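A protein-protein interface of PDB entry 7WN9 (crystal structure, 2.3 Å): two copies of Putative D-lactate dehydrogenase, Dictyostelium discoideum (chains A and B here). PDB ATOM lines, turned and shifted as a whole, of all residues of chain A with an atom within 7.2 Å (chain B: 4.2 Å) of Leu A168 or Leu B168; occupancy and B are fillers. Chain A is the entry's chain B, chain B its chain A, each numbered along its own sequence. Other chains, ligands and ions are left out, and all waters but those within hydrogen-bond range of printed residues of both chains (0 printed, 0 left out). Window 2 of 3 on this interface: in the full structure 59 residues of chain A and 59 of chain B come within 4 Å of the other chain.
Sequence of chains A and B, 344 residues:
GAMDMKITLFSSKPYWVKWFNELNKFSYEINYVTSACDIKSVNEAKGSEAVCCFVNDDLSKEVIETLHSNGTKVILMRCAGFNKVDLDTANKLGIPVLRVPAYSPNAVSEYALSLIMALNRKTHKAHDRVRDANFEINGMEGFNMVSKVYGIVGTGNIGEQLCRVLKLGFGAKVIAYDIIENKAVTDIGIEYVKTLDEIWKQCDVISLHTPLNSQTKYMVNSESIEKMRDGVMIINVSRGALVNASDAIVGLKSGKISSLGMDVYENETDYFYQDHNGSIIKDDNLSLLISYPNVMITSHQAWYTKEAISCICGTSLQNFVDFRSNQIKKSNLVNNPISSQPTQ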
ATOM      1  N   LEU A 162     -10.301  16.810 -14.521  1.00  0.00           N
ATOM      2  CA  LEU A 162     -11.404  16.600 -15.460  1.00  0.00           C
ATOM      3  C   LEU A 162     -12.575  15.888 -14.786  1.00  0.00           C
ATOM      4  O   LEU A 162     -13.737  16.255 -15.004  1.00  0.00           O
ATOM      5  CB  LEU A 162     -10.929  15.804 -16.677  1.00  0.00           C
ATOM      6  CG  LEU A 162     -11.919  15.698 -17.841  1.00  0.00           C
ATOM      7  CD1 LEU A 162     -12.401  17.089 -18.245  1.00  0.00           C
ATOM      8  CD2 LEU A 162     -11.302  14.988 -19.018  1.00  0.00           C
ATOM      9  N   CYS A 163     -12.289  14.861 -13.972  1.00  0.00           N
ATOM     10  CA  CYS A 163     -13.339  14.220 -13.178  1.00  0.00           C
ATOM     11  C   CYS A 163     -14.164  15.257 -12.427  1.00  0.00           C
ATOM     12  O   CYS A 163     -15.397  15.252 -12.486  1.00  0.00           O
ATOM     13  CB  CYS A 163     -12.722  13.226 -12.190  1.00  0.00           C
ATOM     14  SG  CYS A 163     -12.210  11.680 -12.916  1.00  0.00           S
ATOM     15  N   ARG A 164     -13.486  16.176 -11.728  1.00  0.00           N
ATOM     16  CA  ARG A 164     -14.180  17.151 -10.896  1.00  0.00           C
ATOM     17  C   ARG A 164     -15.059  18.066 -11.740  1.00  0.00           C
ATOM     18  O   ARG A 164     -16.215  18.324 -11.394  1.00  0.00           O
ATOM     19  CB  ARG A 164     -13.174  17.976 -10.090  1.00  0.00           C
ATOM     20  CG  ARG A 164     -12.431  17.200  -9.004  1.00  0.00           C
ATOM     21  CD  ARG A 164     -11.530  18.122  -8.148  1.00  0.00           C
ATOM     22  NE  ARG A 164     -12.271  19.246  -7.560  1.00  0.00           N
ATOM     23  CZ  ARG A 164     -12.910  19.210  -6.386  1.00  0.00           C
ATOM     24  NH1 ARG A 164     -12.917  18.100  -5.650  1.00  0.00           N
ATOM     25  NH2 ARG A 164     -13.551  20.288  -5.946  1.00  0.00           N
ATOM     26  N   VAL A 165     -14.521  18.576 -12.850  1.00  0.00           N
ATOM     27  CA  VAL A 165     -15.307  19.462 -13.703  1.00  0.00           C
ATOM     28  C   VAL A 165     -16.556  18.744 -14.204  1.00  0.00           C
ATOM     29  O   VAL A 165     -17.661  19.289 -14.162  1.00  0.00           O
ATOM     30  CB  VAL A 165     -14.446  19.994 -14.863  1.00  0.00           C
ATOM     31  CG1 VAL A 165     -15.300  20.760 -15.829  1.00  0.00           C
ATOM     32  CG2 VAL A 165     -13.361  20.907 -14.311  1.00  0.00           C
ATOM     33  N   LEU A 166     -16.405  17.502 -14.667  1.00  0.00           N
ATOM     34  CA  LEU A 166     -17.551  16.789 -15.217  1.00  0.00           C
ATOM     35  C   LEU A 166     -18.571  16.459 -14.131  1.00  0.00           C
ATOM     36  O   LEU A 166     -19.777  16.667 -14.316  1.00  0.00           O
ATOM     37  CB  LEU A 166     -17.091  15.514 -15.926  1.00  0.00           C
ATOM     38  CG  LEU A 166     -16.226  15.725 -17.175  1.00  0.00           C
ATOM     39  CD1 LEU A 166     -15.639  14.397 -17.648  1.00  0.00           C
ATOM     40  CD2 LEU A 166     -17.041  16.384 -18.289  1.00  0.00           C
ATOM     41  N   LYS A 167     -18.102  15.934 -12.990  1.00  0.00           N
ATOM     42  CA  LYS A 167     -19.003  15.462 -11.940  1.00  0.00           C
ATOM     43  C   LYS A 167     -19.628  16.621 -11.178  1.00  0.00           C
ATOM     44  O   LYS A 167     -20.850  16.676 -11.006  1.00  0.00           O
ATOM     45  CB  LYS A 167     -18.246  14.553 -10.972  1.00  0.00           C
ATOM     46  CG  LYS A 167     -19.099  13.921  -9.866  1.00  0.00           C
ATOM     47  CD  LYS A 167     -20.080  12.923 -10.442  1.00  0.00           C
ATOM     48  CE  LYS A 167     -20.517  11.919  -9.398  1.00  0.00           C
ATOM     49  NZ  LYS A 167     -20.412  12.528  -8.059  1.00  0.00           N
ATOM     50  N   LEU A 168     -18.796  17.547 -10.705  1.00  0.00           N
ATOM     51  CA  LEU A 168     -19.279  18.671  -9.916  1.00  0.00           C
ATOM     52  C   LEU A 168     -19.860  19.784 -10.779  1.00  0.00           C
ATOM     53  O   LEU A 168     -20.812  20.444 -10.358  1.00  0.00           O
ATOM     54  CB  LEU A 168     -18.146  19.224  -9.059  1.00  0.00           C
ATOM     55  CG  LEU A 168     -17.487  18.197  -8.142  1.00  0.00           C
ATOM     56  CD1 LEU A 168     -16.351  18.837  -7.367  1.00  0.00           C
ATOM     57  CD2 LEU A 168     -18.526  17.585  -7.196  1.00  0.00           C
ATOM     58  N   GLY A 169     -19.305  20.019 -11.967  1.00  0.00           N
ATOM     59  CA  GLY A 169     -19.788  21.081 -12.828  1.00  0.00           C
ATOM     60  C   GLY A 169     -21.083  20.764 -13.553  1.00  0.00           C
ATOM     61  O   GLY A 169     -21.958  21.623 -13.652  1.00  0.00           O
ATOM     62  N   PHE A 170     -21.221  19.548 -14.078  1.00  0.00           N
ATOM     63  CA  PHE A 170     -22.407  19.162 -14.833  1.00  0.00           C
ATOM     64  C   PHE A 170     -23.251  18.105 -14.144  1.00  0.00           C
ATOM     65  O   PHE A 170     -24.300  17.731 -14.678  1.00  0.00           O
ATOM     66  CB  PHE A 170     -22.010  18.634 -16.216  1.00  0.00           C
ATOM     67  CG  PHE A 170     -21.154  19.582 -16.993  1.00  0.00           C
ATOM     68  CD1 PHE A 170     -19.800  19.340 -17.152  1.00  0.00           C
ATOM     69  CD2 PHE A 170     -21.703  20.723 -17.555  1.00  0.00           C
ATOM     70  CE1 PHE A 170     -19.007  20.213 -17.873  1.00  0.00           C
ATOM     71  CE2 PHE A 170     -20.922  21.601 -18.269  1.00  0.00           C
ATOM     72  CZ  PHE A 170     -19.566  21.347 -18.430  1.00  0.00           C
ATOM     73  N   GLY A 171     -22.807  17.584 -13.002  1.00  0.00           N
ATOM     74  CA  GLY A 171     -23.505  16.474 -12.382  1.00  0.00           C
ATOM     75  C   GLY A 171     -23.530  15.211 -13.209  1.00  0.00           C
ATOM     76  O   GLY A 171     -24.437  14.399 -13.045  1.00  0.00           O
ATOM     77  N   ALA A 172     -22.561  15.019 -14.103  1.00  0.00           N
ATOM     78  CA  ALA A 172     -22.578  13.846 -14.967  1.00  0.00           C
ATOM     79  C   ALA A 172     -22.100  12.599 -14.226  1.00  0.00           C
ATOM     80  O   ALA A 172     -21.387  12.670 -13.228  1.00  0.00           O
ATOM     81  CB  ALA A 172     -21.694  14.074 -16.193  1.00  0.00           C
ATOM     82  N   VAL A 174     -19.489   9.871 -14.043  1.00  0.00           N
ATOM     83  CA  VAL A 174     -18.101   9.651 -14.429  1.00  0.00           C
ATOM     84  C   VAL A 174     -17.652   8.300 -13.890  1.00  0.00           C
ATOM     85  O   VAL A 174     -17.905   7.980 -12.723  1.00  0.00           O
ATOM     86  CB  VAL A 174     -17.181  10.768 -13.888  1.00  0.00           C
ATOM     87  CG1 VAL A 174     -15.750  10.552 -14.372  1.00  0.00           C
ATOM     88  CG2 VAL A 174     -17.700  12.140 -14.313  1.00  0.00           C
ATOM     89  N   ILE A 188     -15.495  12.282  -4.283  1.00  0.00           N
ATOM     90  CA  ILE A 188     -16.639  12.946  -4.893  1.00  0.00           C
ATOM     91  C   ILE A 188     -17.572  11.934  -5.554  1.00  0.00           C
ATOM     92  O   ILE A 188     -18.360  12.293  -6.426  1.00  0.00           O
ATOM     93  CB  ILE A 188     -16.217  14.054  -5.873  1.00  0.00           C
ATOM     94  CG1 ILE A 188     -15.340  13.496  -6.999  1.00  0.00           C
ATOM     95  CG2 ILE A 188     -15.490  15.171  -5.120  1.00  0.00           C
ATOM     96  CD1 ILE A 188     -14.897  14.540  -7.994  1.00  0.00           C
ATOM     97  N   ILE A 190     -17.078   9.121  -7.431  1.00  0.00           N
ATOM     98  CA  ILE A 190     -16.795   8.532  -8.732  1.00  0.00           C
ATOM     99  C   ILE A 190     -16.284   7.116  -8.519  1.00  0.00           C
ATOM    100  O   ILE A 190     -15.367   6.884  -7.722  1.00  0.00           O
ATOM    101  CB  ILE A 190     -15.787   9.392  -9.512  1.00  0.00           C
ATOM    102  CG1 ILE A 190     -16.489  10.662 -10.015  1.00  0.00           C
ATOM    103  CG2 ILE A 190     -15.159   8.589 -10.654  1.00  0.00           C
ATOM    104  CD1 ILE A 190     -15.538  11.766 -10.503  1.00  0.00           C
ATOM    105  N   ARG B 164     -23.728  27.727 -11.733  1.00  0.00           N
ATOM    106  CA  ARG B 164     -23.330  26.475 -11.102  1.00  0.00           C
ATOM    107  C   ARG B 164     -22.131  25.851 -11.800  1.00  0.00           C
ATOM    108  O   ARG B 164     -21.221  25.341 -11.139  1.00  0.00           O
ATOM    109  CB  ARG B 164     -24.500  25.490 -11.091  1.00  0.00           C
ATOM    110  CG  ARG B 164     -25.674  25.927 -10.215  1.00  0.00           C
ATOM    111  CD  ARG B 164     -26.832  24.919 -10.283  1.00  0.00           C
ATOM    112  NE  ARG B 164     -26.405  23.608  -9.800  1.00  0.00           N
ATOM    113  CZ  ARG B 164     -26.355  23.263  -8.513  1.00  0.00           C
ATOM    114  NH1 ARG B 164     -26.713  24.132  -7.565  1.00  0.00           N
ATOM    115  NH2 ARG B 164     -25.945  22.046  -8.177  1.00  0.00           N
ATOM    116  N   VAL B 165     -22.119  25.856 -13.133  1.00  0.00           N
ATOM    117  CA  VAL B 165     -21.004  25.249 -13.856  1.00  0.00           C
ATOM    118  C   VAL B 165     -19.701  25.962 -13.517  1.00  0.00           C
ATOM    119  O   VAL B 165     -18.673  25.329 -13.246  1.00  0.00           O
ATOM    120  CB  VAL B 165     -21.272  25.278 -15.370  1.00  0.00           C
ATOM    121  CG1 VAL B 165     -20.029  24.840 -16.109  1.00  0.00           C
ATOM    122  CG2 VAL B 165     -22.435  24.383 -15.696  1.00  0.00           C
ATOM    123  N   LEU B 166     -19.723  27.295 -13.543  1.00  0.00           N
ATOM    124  CA  LEU B 166     -18.515  28.071 -13.300  1.00  0.00           C
ATOM    125  C   LEU B 166     -18.043  27.924 -11.855  1.00  0.00           C
ATOM    126  O   LEU B 166     -16.851  27.711 -11.594  1.00  0.00           O
ATOM    127  CB  LEU B 166     -18.782  29.538 -13.640  1.00  0.00           C
ATOM    128  CG  LEU B 166     -19.083  29.850 -15.116  1.00  0.00           C
ATOM    129  CD1 LEU B 166     -19.562  31.300 -15.301  1.00  0.00           C
ATOM    130  CD2 LEU B 166     -17.848  29.570 -15.979  1.00  0.00           C
ATOM    131  N   LYS B 167     -18.967  28.035 -10.903  1.00  0.00           N
ATOM    132  CA  LYS B 167     -18.622  28.016  -9.487  1.00  0.00           C
ATOM    133  C   LYS B 167     -18.288  26.610  -9.014  1.00  0.00           C
ATOM    134  O   LYS B 167     -17.231  26.380  -8.424  1.00  0.00           O
ATOM    135  CB  LYS B 167     -19.781  28.586  -8.664  1.00  0.00           C
ATOM    136  CG  LYS B 167     -19.564  28.550  -7.167  1.00  0.00           C
ATOM    137  CD  LYS B 167     -18.657  29.674  -6.717  1.00  0.00           C
ATOM    138  CE  LYS B 167     -18.578  29.702  -5.195  1.00  0.00           C
ATOM    139  NZ  LYS B 167     -18.150  31.049  -4.700  1.00  0.00           N
ATOM    140  N   LEU B 168     -19.183  25.661  -9.247  1.00  0.00           N
ATOM    141  CA  LEU B 168     -18.966  24.310  -8.755  1.00  0.00           C
ATOM    142  C   LEU B 168     -18.015  23.520  -9.639  1.00  0.00           C
ATOM    143  O   LEU B 168     -17.299  22.652  -9.137  1.00  0.00           O
ATOM    144  CB  LEU B 168     -20.298  23.573  -8.645  1.00  0.00           C
ATOM    145  CG  LEU B 168     -21.370  24.303  -7.842  1.00  0.00           C
ATOM    146  CD1 LEU B 168     -22.673  23.489  -7.826  1.00  0.00           C
ATOM    147  CD2 LEU B 168     -20.848  24.564  -6.426  1.00  0.00           C
ATOM    148  N   GLY B 169     -17.998  23.784 -10.944  1.00  0.00           N
ATOM    149  CA  GLY B 169     -17.149  23.019 -11.836  1.00  0.00           C
ATOM    150  C   GLY B 169     -15.703  23.472 -11.850  1.00  0.00           C
ATOM    151  O   GLY B 169     -14.793  22.643 -11.864  1.00  0.00           O
ATOM    152  N   PHE B 170     -15.469  24.782 -11.861  1.00  0.00           N
ATOM    153  CA  PHE B 170     -14.118  25.319 -11.898  1.00  0.00           C
ATOM    154  C   PHE B 170     -13.728  26.019 -10.608  1.00  0.00           C
ATOM    155  O   PHE B 170     -12.583  26.465 -10.487  1.00  0.00           O
ATOM    156  CB  PHE B 170     -13.963  26.300 -13.070  1.00  0.00           C
ATOM    157  CG  PHE B 170     -14.342  25.720 -14.395  1.00  0.00           C
ATOM    158  CD1 PHE B 170     -13.505  24.815 -15.031  1.00  0.00           C
ATOM    159  CD2 PHE B 170     -15.526  26.078 -15.005  1.00  0.00           C
ATOM    160  CE1 PHE B 170     -13.851  24.271 -16.256  1.00  0.00           C
ATOM    161  CE2 PHE B 170     -15.878  25.544 -16.234  1.00  0.00           C
ATOM    162  CZ  PHE B 170     -15.034  24.635 -16.863  1.00  0.00           C
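Hydrophobic or aromatic side chains of chain B within 4 Å of the printed part of chain A: Val B165, Leu B168 and Phe B170.
Of the printed residues of chain B, Val A165 touches Gly B169 and Phe B170.
Leu A168 touches just one residue of chain B: Leu B168 (3.5 Å).
Ala A172 touches none of the printed residues of chain B.
Of the printed residues of chain A, Val B165 touches Gly A169 and Phe A170.
Leu B166 touches none of the printed residues of chain A.
Leu B168 touches just one residue of chain A: Leu A168 (3.5 Å).
Printed residues of chain A within 4 Å of Gly B169: Val A165 and Gly A169.
Of the printed residues of chain A, Phe B170 touches Val A165 (3.8 Å).
The nearest printed residue of chain B that does not touch Leu A168 is Gly B169 (4.4 Å).
The nearest printed residue of chain A that does not touch Val B165 is Leu A168 (5.9 Å).
Among the printed residues, pairs that only touch across the chains: Val A165 with Gly B169, Val A165 with Phe B170, Leu A168 with Leu B168, Gly A169 with Val B165, Gly A169 with Gly B169 and Phe A170 with Val B165.
Val A165 touches Gly B169, and with the chains exchanged Gly A169 touches Val B165.
Val A165 touches Phe B170, and with the chains exchanged Phe A170 touches Val B165.
Leu B168 touches its own counterpart, Leu A168.
Gly A169 touches its own counterpart, Gly B169.
7 positions are printed for both chains.
Of the 6 pairs that touch across the chains among the printed residues, 6 have their exchanged pair printed and touching as well.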
